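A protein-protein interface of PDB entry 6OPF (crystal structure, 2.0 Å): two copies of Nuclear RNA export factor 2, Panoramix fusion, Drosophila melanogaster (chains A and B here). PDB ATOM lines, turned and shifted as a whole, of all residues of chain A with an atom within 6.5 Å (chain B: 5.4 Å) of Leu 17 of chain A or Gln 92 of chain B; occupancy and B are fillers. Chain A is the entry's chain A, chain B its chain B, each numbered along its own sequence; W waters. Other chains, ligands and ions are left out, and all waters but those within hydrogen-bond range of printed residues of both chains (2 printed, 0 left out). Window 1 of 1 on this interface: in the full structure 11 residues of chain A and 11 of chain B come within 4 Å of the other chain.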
ATOM      1  N   VAL A  10     -18.226  28.101  -6.779  1.00  0.00           N
ATOM      2  CA  VAL A  10     -17.847  28.440  -8.146  1.00  0.00           C
ATOM      3  C   VAL A  10     -16.327  28.548  -8.260  1.00  0.00           C
ATOM      4  O   VAL A  10     -15.725  28.053  -9.221  1.00  0.00           O
ATOM      5  CB  VAL A  10     -18.548  29.741  -8.583  1.00  0.00           C
ATOM      6  CG1 VAL A  10     -17.863  30.354  -9.812  1.00  0.00           C
ATOM      7  CG2 VAL A  10     -20.025  29.487  -8.844  1.00  0.00           C
ATOM      8  N   ASP A  12     -14.110  27.039  -6.319  1.00  0.00           N
ATOM      9  CA  ASP A  12     -13.567  25.700  -6.132  1.00  0.00           C
ATOM     10  C   ASP A  12     -13.654  24.890  -7.428  1.00  0.00           C
ATOM     11  O   ASP A  12     -12.720  24.154  -7.778  1.00  0.00           O
ATOM     12  CB  ASP A  12     -14.321  25.029  -4.972  1.00  0.00           C
ATOM     13  CG  ASP A  12     -13.813  23.639  -4.651  1.00  0.00           C
ATOM     14  OD1 ASP A  12     -12.767  23.508  -3.961  1.00  0.00           O
ATOM     15  OD2 ASP A  12     -14.482  22.665  -5.080  1.00  0.00           O
ATOM     16  N   HIS A  13     -14.750  25.044  -8.181  1.00  0.00           N
ATOM     17  CA  HIS A  13     -14.873  24.309  -9.437  1.00  0.00           C
ATOM     18  C   HIS A  13     -14.004  24.903 -10.536  1.00  0.00           C
ATOM     19  O   HIS A  13     -13.566  24.170 -11.433  1.00  0.00           O
ATOM     20  CB  HIS A  13     -16.334  24.266  -9.881  1.00  0.00           C
ATOM     21  CG  HIS A  13     -17.145  23.238  -9.159  1.00  0.00           C
ATOM     22  ND1 HIS A  13     -18.478  23.013  -9.431  1.00  0.00           N
ATOM     23  CD2 HIS A  13     -16.810  22.365  -8.181  1.00  0.00           C
ATOM     24  CE1 HIS A  13     -18.932  22.054  -8.642  1.00  0.00           C
ATOM     25  NE2 HIS A  13     -17.940  21.644  -7.874  1.00  0.00           N
ATOM     26  N   LYS A  14     -13.754  26.218 -10.499  1.00  0.00           N
ATOM     27  CA  LYS A  14     -12.841  26.798 -11.480  1.00  0.00           C
ATOM     28  C   LYS A  14     -11.442  26.240 -11.289  1.00  0.00           C
ATOM     29  O   LYS A  14     -10.771  25.870 -12.258  1.00  0.00           O
ATOM     30  CB  LYS A  14     -12.824  28.325 -11.368  1.00  0.00           C
ATOM     31  CG  LYS A  14     -13.845  29.036 -12.241  1.00  0.00           C
ATOM     32  CD  LYS A  14     -14.010  30.491 -11.802  1.00  0.00           C
ATOM     33  CE  LYS A  14     -15.069  31.209 -12.621  1.00  0.00           C
ATOM     34  NZ  LYS A  14     -15.300  32.618 -12.148  1.00  0.00           N
ATOM     35  N   LEU A  15     -10.997  26.165 -10.033  1.00  0.00           N
ATOM     36  CA  LEU A  15      -9.692  25.598  -9.713  1.00  0.00           C
ATOM     37  C   LEU A  15      -9.603  24.138 -10.141  1.00  0.00           C
ATOM     38  O   LEU A  15      -8.623  23.718 -10.770  1.00  0.00           O
ATOM     39  CB  LEU A  15      -9.434  25.729  -8.208  1.00  0.00           C
ATOM     40  CG  LEU A  15      -9.304  27.158  -7.692  1.00  0.00           C
ATOM     41  CD1 LEU A  15      -9.245  27.125  -6.174  1.00  0.00           C
ATOM     42  CD2 LEU A  15      -8.041  27.836  -8.287  1.00  0.00           C
ATOM     43  N   LEU A  16     -10.616  23.342  -9.779  1.00  0.00           N
ATOM     44  CA  LEU A  16     -10.587  21.926 -10.110  1.00  0.00           C
ATOM     45  C   LEU A  16     -10.507  21.716 -11.619  1.00  0.00           C
ATOM     46  O   LEU A  16      -9.719  20.894 -12.096  1.00  0.00           O
ATOM     47  CB  LEU A  16     -11.819  21.224  -9.514  1.00  0.00           C
ATOM     48  CG  LEU A  16     -11.807  19.696  -9.534  1.00  0.00           C
ATOM     49  CD1 LEU A  16     -10.668  19.145  -8.694  1.00  0.00           C
ATOM     50  CD2 LEU A  16     -13.148  19.159  -9.015  1.00  0.00           C
ATOM     51  N   LEU A  17     -11.295  22.466 -12.395  1.00  0.00           N
ATOM     52  CA  LEU A  17     -11.240  22.287 -13.844  1.00  0.00           C
ATOM     53  C   LEU A  17      -9.909  22.779 -14.407  1.00  0.00           C
ATOM     54  O   LEU A  17      -9.339  22.160 -15.323  1.00  0.00           O
ATOM     55  CB  LEU A  17     -12.405  23.008 -14.523  1.00  0.00           C
ATOM     56  CG  LEU A  17     -12.389  22.800 -16.048  1.00  0.00           C
ATOM     57  CD1 LEU A  17     -12.686  21.353 -16.404  1.00  0.00           C
ATOM     58  CD2 LEU A  17     -13.370  23.706 -16.747  1.00  0.00           C
ATOM     59  N   PHE A  18      -9.391  23.881 -13.864  1.00  0.00           N
ATOM     60  CA  PHE A  18      -8.081  24.349 -14.307  1.00  0.00           C
ATOM     61  C   PHE A  18      -7.013  23.295 -14.036  1.00  0.00           C
ATOM     62  O   PHE A  18      -6.171  23.029 -14.897  1.00  0.00           O
ATOM     63  CB  PHE A  18      -7.739  25.674 -13.620  1.00  0.00           C
ATOM     64  CG  PHE A  18      -6.586  26.408 -14.267  1.00  0.00           C
ATOM     65  CD1 PHE A  18      -6.803  27.224 -15.368  1.00  0.00           C
ATOM     66  CD2 PHE A  18      -5.304  26.281 -13.780  1.00  0.00           C
ATOM     67  CE1 PHE A  18      -5.748  27.910 -15.979  1.00  0.00           C
ATOM     68  CE2 PHE A  18      -4.230  26.970 -14.390  1.00  0.00           C
ATOM     69  CZ  PHE A  18      -4.474  27.767 -15.489  1.00  0.00           C
ATOM     70  N   GLN A  19      -7.066  22.646 -12.864  1.00  0.00           N
ATOM     71  CA  GLN A  19      -6.138  21.552 -12.569  1.00  0.00           C
ATOM     72  C   GLN A  19      -6.303  20.380 -13.543  1.00  0.00           C
ATOM     73  O   GLN A  19      -5.310  19.803 -14.004  1.00  0.00           O
ATOM     74  CB  GLN A  19      -6.336  21.083 -11.131  1.00  0.00           C
ATOM     75  CG  GLN A  19      -5.286  20.074 -10.649  1.00  0.00           C
ATOM     76  CD  GLN A  19      -5.196  19.994  -9.132  1.00  0.00           C
ATOM     77  OE1 GLN A  19      -6.112  19.510  -8.486  1.00  0.00           O
ATOM     78  NE2 GLN A  19      -4.088  20.489  -8.556  1.00  0.00           N
ATOM     79  N   GLU A  20      -7.552  20.001 -13.861  1.00  0.00           N
ATOM     80  CA  GLU A  20      -7.755  18.900 -14.803  1.00  0.00           C
ATOM     81  C   GLU A  20      -7.243  19.253 -16.200  1.00  0.00           C
ATOM     82  O   GLU A  20      -6.655  18.402 -16.877  1.00  0.00           O
ATOM     83  CB  GLU A  20      -9.233  18.493 -14.818  1.00  0.00           C
ATOM     84  CG  GLU A  20      -9.565  17.638 -13.600  1.00  0.00           C
ATOM     85  CD  GLU A  20     -11.060  17.346 -13.437  1.00  0.00           C
ATOM     86  OE1 GLU A  20     -11.813  17.503 -14.423  1.00  0.00           O
ATOM     87  OE2 GLU A  20     -11.469  16.964 -12.316  1.00  0.00           O
ATOM     88  N   VAL A  21      -7.387  20.512 -16.617  1.00  0.00           N
ATOM     89  CA  VAL A  21      -6.890  20.931 -17.925  1.00  0.00           C
ATOM     90  C   VAL A  21      -5.361  20.915 -17.968  1.00  0.00           C
ATOM     91  O   VAL A  21      -4.760  20.417 -18.931  1.00  0.00           O
ATOM     92  CB  VAL A  21      -7.450  22.323 -18.276  1.00  0.00           C
ATOM     93  CG1 VAL A  21      -6.702  22.931 -19.457  1.00  0.00           C
ATOM     94  CG2 VAL A  21      -8.956  22.264 -18.523  1.00  0.00           C
ATOM     95  N   THR A  22      -4.702  21.463 -16.930  1.00  0.00           N
ATOM     96  CA  THR A  22      -3.271  21.753 -17.018  1.00  0.00           C
ATOM     97  C   THR A  22      -2.350  20.697 -16.419  1.00  0.00           C
ATOM     98  O   THR A  22      -1.152  20.701 -16.740  1.00  0.00           O
ATOM     99  CB  THR A  22      -2.950  23.074 -16.316  1.00  0.00           C
ATOM    100  OG1 THR A  22      -3.334  22.977 -14.938  1.00  0.00           O
ATOM    101  CG2 THR A  22      -3.663  24.233 -16.997  1.00  0.00           C
ATOM    102  N   TRP A  38      -9.907  35.086 -11.212  1.00  0.00           N
ATOM    103  CA  TRP A  38     -10.964  34.083 -11.284  1.00  0.00           C
ATOM    104  C   TRP A  38     -11.643  34.052 -12.644  1.00  0.00           C
ATOM    105  O   TRP A  38     -12.700  33.430 -12.789  1.00  0.00           O
ATOM    106  CB  TRP A  38     -11.989  34.293 -10.160  1.00  0.00           C
ATOM    107  CG  TRP A  38     -11.293  34.273  -8.856  1.00  0.00           C
ATOM    108  CD1 TRP A  38     -10.902  35.346  -8.118  1.00  0.00           C
ATOM    109  CD2 TRP A  38     -10.821  33.112  -8.167  1.00  0.00           C
ATOM    110  NE1 TRP A  38     -10.240  34.925  -6.993  1.00  0.00           N
ATOM    111  CE2 TRP A  38     -10.171  33.556  -7.001  1.00  0.00           C
ATOM    112  CE3 TRP A  38     -10.906  31.732  -8.415  1.00  0.00           C
ATOM    113  CZ2 TRP A  38      -9.609  32.675  -6.074  1.00  0.00           C
ATOM    114  CZ3 TRP A  38     -10.337  30.855  -7.499  1.00  0.00           C
ATOM    115  CH2 TRP A  38      -9.703  31.332  -6.341  1.00  0.00           C
ATOM    116  N   PHE A  40     -11.743  32.363 -15.938  1.00  0.00           N
ATOM    117  CA  PHE A  40     -11.215  31.087 -16.418  1.00  0.00           C
ATOM    118  C   PHE A  40     -10.496  31.252 -17.750  1.00  0.00           C
ATOM    119  O   PHE A  40      -9.391  30.727 -17.942  1.00  0.00           O
ATOM    120  CB  PHE A  40     -12.343  30.051 -16.545  1.00  0.00           C
ATOM    121  CG  PHE A  40     -11.845  28.654 -16.788  1.00  0.00           C
ATOM    122  CD1 PHE A  40     -11.275  27.920 -15.754  1.00  0.00           C
ATOM    123  CD2 PHE A  40     -11.924  28.078 -18.043  1.00  0.00           C
ATOM    124  CE1 PHE A  40     -10.791  26.642 -15.964  1.00  0.00           C
ATOM    125  CE2 PHE A  40     -11.452  26.789 -18.261  1.00  0.00           C
ATOM    126  CZ  PHE A  40     -10.873  26.076 -17.213  1.00  0.00           C
ATOM    127  N   VAL A  89      -9.365  23.988 -25.046  1.00  0.00           N
ATOM    128  CA  VAL A  89     -10.446  24.572 -24.258  1.00  0.00           C
ATOM    129  C   VAL A  89     -10.575  26.060 -24.570  1.00  0.00           C
ATOM    130  O   VAL A  89     -11.687  26.598 -24.671  1.00  0.00           O
ATOM    131  CB  VAL A  89     -10.215  24.315 -22.750  1.00  0.00           C
ATOM    132  CG1 VAL A  89     -11.232  25.052 -21.902  1.00  0.00           C
ATOM    133  CG2 VAL A  89     -10.257  22.806 -22.430  1.00  0.00           C
ATOM    134  N   ILE A  93     -14.126  28.452 -25.445  1.00  0.00           N
ATOM    135  CA  ILE A  93     -14.623  29.612 -24.715  1.00  0.00           C
ATOM    136  C   ILE A  93     -14.822  30.777 -25.669  1.00  0.00           C
ATOM    137  O   ILE A  93     -15.808  31.517 -25.576  1.00  0.00           O
ATOM    138  CB  ILE A  93     -13.665  29.979 -23.566  1.00  0.00           C
ATOM    139  CG1 ILE A  93     -13.587  28.850 -22.540  1.00  0.00           C
ATOM    140  CG2 ILE A  93     -14.106  31.275 -22.888  1.00  0.00           C
ATOM    141  CD1 ILE A  93     -12.547  29.104 -21.475  1.00  0.00           C
ATOM    142  N   GLU B  87     -20.263  17.998 -16.866  1.00  0.00           N
ATOM    143  CA  GLU B  87     -20.919  18.952 -15.978  1.00  0.00           C
ATOM    144  C   GLU B  87     -19.946  20.026 -15.511  1.00  0.00           C
ATOM    145  O   GLU B  87     -20.319  21.196 -15.394  1.00  0.00           O
ATOM    146  CB  GLU B  87     -21.572  18.217 -14.802  1.00  0.00           C
ATOM    147  CG  GLU B  87     -22.921  17.587 -15.216  1.00  0.00           C
ATOM    148  CD  GLU B  87     -23.545  16.674 -14.171  1.00  0.00           C
ATOM    149  OE1 GLU B  87     -22.813  16.182 -13.280  1.00  0.00           O
ATOM    150  OE2 GLU B  87     -24.778  16.435 -14.254  1.00  0.00           O
ATOM    151  N   LEU B  88     -18.680  19.662 -15.308  1.00  0.00           N
ATOM    152  CA  LEU B  88     -17.687  20.639 -14.861  1.00  0.00           C
ATOM    153  C   LEU B  88     -17.385  21.654 -15.957  1.00  0.00           C
ATOM    154  O   LEU B  88     -17.309  22.859 -15.700  1.00  0.00           O
ATOM    155  CB  LEU B  88     -16.424  19.905 -14.417  1.00  0.00           C
ATOM    156  CG  LEU B  88     -15.416  20.590 -13.494  1.00  0.00           C
ATOM    157  CD1 LEU B  88     -16.060  21.089 -12.195  1.00  0.00           C
ATOM    158  CD2 LEU B  88     -14.285  19.622 -13.211  1.00  0.00           C
ATOM    159  N   VAL B  89     -17.219  21.185 -17.197  1.00  0.00           N
ATOM    160  CA  VAL B  89     -17.031  22.103 -18.317  1.00  0.00           C
ATOM    161  C   VAL B  89     -18.271  22.969 -18.508  1.00  0.00           C
ATOM    162  O   VAL B  89     -18.169  24.183 -18.722  1.00  0.00           O
ATOM    163  CB  VAL B  89     -16.680  21.322 -19.602  1.00  0.00           C
ATOM    164  CG1 VAL B  89     -16.552  22.259 -20.801  1.00  0.00           C
ATOM    165  CG2 VAL B  89     -15.395  20.513 -19.411  1.00  0.00           C
ATOM    166  N   LEU B  90     -19.461  22.353 -18.467  1.00  0.00           N
ATOM    167  CA  LEU B  90     -20.709  23.089 -18.625  1.00  0.00           C
ATOM    168  C   LEU B  90     -20.778  24.299 -17.699  1.00  0.00           C
ATOM    169  O   LEU B  90     -21.068  25.414 -18.139  1.00  0.00           O
ATOM    170  CB  LEU B  90     -21.901  22.168 -18.358  1.00  0.00           C
ATOM    171  CG  LEU B  90     -22.865  21.974 -19.511  1.00  0.00           C
ATOM    172  CD1 LEU B  90     -24.082  21.210 -18.999  1.00  0.00           C
ATOM    173  CD2 LEU B  90     -23.268  23.313 -20.119  1.00  0.00           C
ATOM    174  N   GLU B  91     -20.558  24.078 -16.401  1.00  0.00           N
ATOM    175  CA  GLU B  91     -20.510  25.170 -15.431  1.00  0.00           C
ATOM    176  C   GLU B  91     -19.666  26.331 -15.930  1.00  0.00           C
ATOM    177  O   GLU B  91     -20.104  27.485 -15.915  1.00  0.00           O
ATOM    178  CB  GLU B  91     -19.954  24.666 -14.100  1.00  0.00           C
ATOM    179  CG  GLU B  91     -20.971  23.958 -13.241  1.00  0.00           C
ATOM    180  CD  GLU B  91     -20.324  23.263 -12.057  1.00  0.00           C
ATOM    181  OE1 GLU B  91     -19.338  23.827 -11.506  1.00  0.00           O
ATOM    182  OE2 GLU B  91     -20.803  22.160 -11.689  1.00  0.00           O
ATOM    183  N   GLN B  92     -18.459  26.028 -16.407  1.00  0.00           N
ATOM    184  CA  GLN B  92     -17.524  27.073 -16.803  1.00  0.00           C
ATOM    185  C   GLN B  92     -17.993  27.815 -18.040  1.00  0.00           C
ATOM    186  O   GLN B  92     -17.802  29.032 -18.147  1.00  0.00           O
ATOM    187  CB  GLN B  92     -16.146  26.472 -17.034  1.00  0.00           C
ATOM    188  CG  GLN B  92     -15.464  26.143 -15.740  1.00  0.00           C
ATOM    189  CD  GLN B  92     -15.657  27.240 -14.715  1.00  0.00           C
ATOM    190  OE1 GLN B  92     -16.120  26.986 -13.603  1.00  0.00           O
ATOM    191  NE2 GLN B  92     -15.316  28.477 -15.093  1.00  0.00           N
ATOM    192  N   ILE B  93     -18.579  27.092 -18.997  1.00  0.00           N
ATOM    193  CA  ILE B  93     -19.171  27.729 -20.168  1.00  0.00           C
ATOM    194  C   ILE B  93     -20.268  28.689 -19.749  1.00  0.00           C
ATOM    195  O   ILE B  93     -20.403  29.781 -20.315  1.00  0.00           O
ATOM    196  CB  ILE B  93     -19.704  26.658 -21.143  1.00  0.00           C
ATOM    197  CG1 ILE B  93     -18.559  25.805 -21.682  1.00  0.00           C
ATOM    198  CG2 ILE B  93     -20.484  27.312 -22.286  1.00  0.00           C
ATOM    199  CD1 ILE B  93     -18.922  25.083 -22.950  1.00  0.00           C
ATOM    200  N   GLN B  94     -21.044  28.318 -18.735  1.00  0.00           N
ATOM    201  CA  GLN B  94     -22.230  29.067 -18.352  1.00  0.00           C
ATOM    202  C   GLN B  94     -21.939  30.324 -17.533  1.00  0.00           C
ATOM    203  O   GLN B  94     -22.873  31.087 -17.262  1.00  0.00           O
ATOM    204  CB  GLN B  94     -23.187  28.140 -17.604  1.00  0.00           C
ATOM    205  CG  GLN B  94     -23.723  27.030 -18.508  1.00  0.00           C
ATOM    206  CD  GLN B  94     -24.734  26.134 -17.825  1.00  0.00           C
ATOM    207  OE1 GLN B  94     -24.625  25.840 -16.623  1.00  0.00           O
ATOM    208  NE2 GLN B  94     -25.723  25.677 -18.591  1.00  0.00           N
ATOM    209  N   GLN B  95     -20.717  30.439 -17.022  1.00  0.00           N
ATOM    210  CA  GLN B  95     -20.299  31.641 -16.267  1.00  0.00           C
ATOM    211  C   GLN B  95     -19.706  32.612 -17.286  1.00  0.00           C
ATOM    212  O   GLN B  95     -18.587  32.326 -17.713  1.00  0.00           O
ATOM    213  CB  GLN B  95     -19.199  31.343 -15.253  1.00  0.00           C
ATOM    214  CG  GLN B  95     -19.431  30.181 -14.297  1.00  0.00           C
ATOM    215  CD  GLN B  95     -20.258  30.570 -13.098  1.00  0.00           C
ATOM    216  OE1 GLN B  95     -20.037  31.596 -12.461  1.00  0.00           O
ATOM    217  NE2 GLN B  95     -21.248  29.755 -12.789  1.00  0.00           N
HETATM  218  O   HOH W   1     -18.028  33.072 -12.881  1.00  0.00           O
HETATM  219  O   HOH W   2     -17.212  27.348 -11.480  1.00  0.00           O
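OE2 of Glu 91 of chain B lies close to ND1 of His 13 of chain A.
The side-chain amino group (NZ) of Lys 14 of chain A is in hydrogen-bond range of the backbone carbonyl oxygen (O) of Trp 38 of chain A.
Among the printed residues, merely in contact across the chains: Lys 14 of chain A with Gln 92 of chain B, Leu 17 of chain A with Gln 92 of chain B, Glu 20 of chain A with Leu 88 of chain B, Val 10 of chain A with Gln 95 of chain B, Phe 40 of chain A with Gln 92 of chain B, His 13 of chain A with Leu 88 of chain B and Leu 17 of chain A with Leu 88 of chain B.
Of the printed residues of chain B, His 13 of chain A touches Leu 88 (3.9 Å) and Glu 91 (2.4 Å).
Of the printed residues of chain B, Leu 17 of chain A touches Leu 88 (3.97 Å) and Gln 92 (3.4 Å).
Of the printed residues of chain B, Glu 20 of chain A touches Leu 88 (3.5 Å).
Printed residues of chain B within 4 Å of Phe 40 of chain A: Gln 92 (3.7 Å).
Of the printed residues of chain A, Leu 88 of chain B touches His 13 (3.9 Å), Leu 17 (3.97 Å) and Glu 20 (3.5 Å).
Hydrophobic or aromatic side chains of chain B that line the printed part of chain A: Leu 88.
Among the printed residues, no Asp or Glu carboxylate lies within 4 Å of a Lys or Arg side-chain nitrogen of the other chain.
2 positions are printed for both chains.
Of the 8 pairs that touch across the chains among the printed residues, none has its exchanged pair printed and touching as well.
Water W2 bridges OE1 of Gln 92 of chain B (2.4 Å) and O of Val 10 of chain A (2.8 Å).
Water W1 bridges the side-chain amide oxygen (OE1) of Gln 95 of chain B (2.5 Å) and the side-chain amino group (NZ) of Lys 14 of chain A (2.9 Å).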
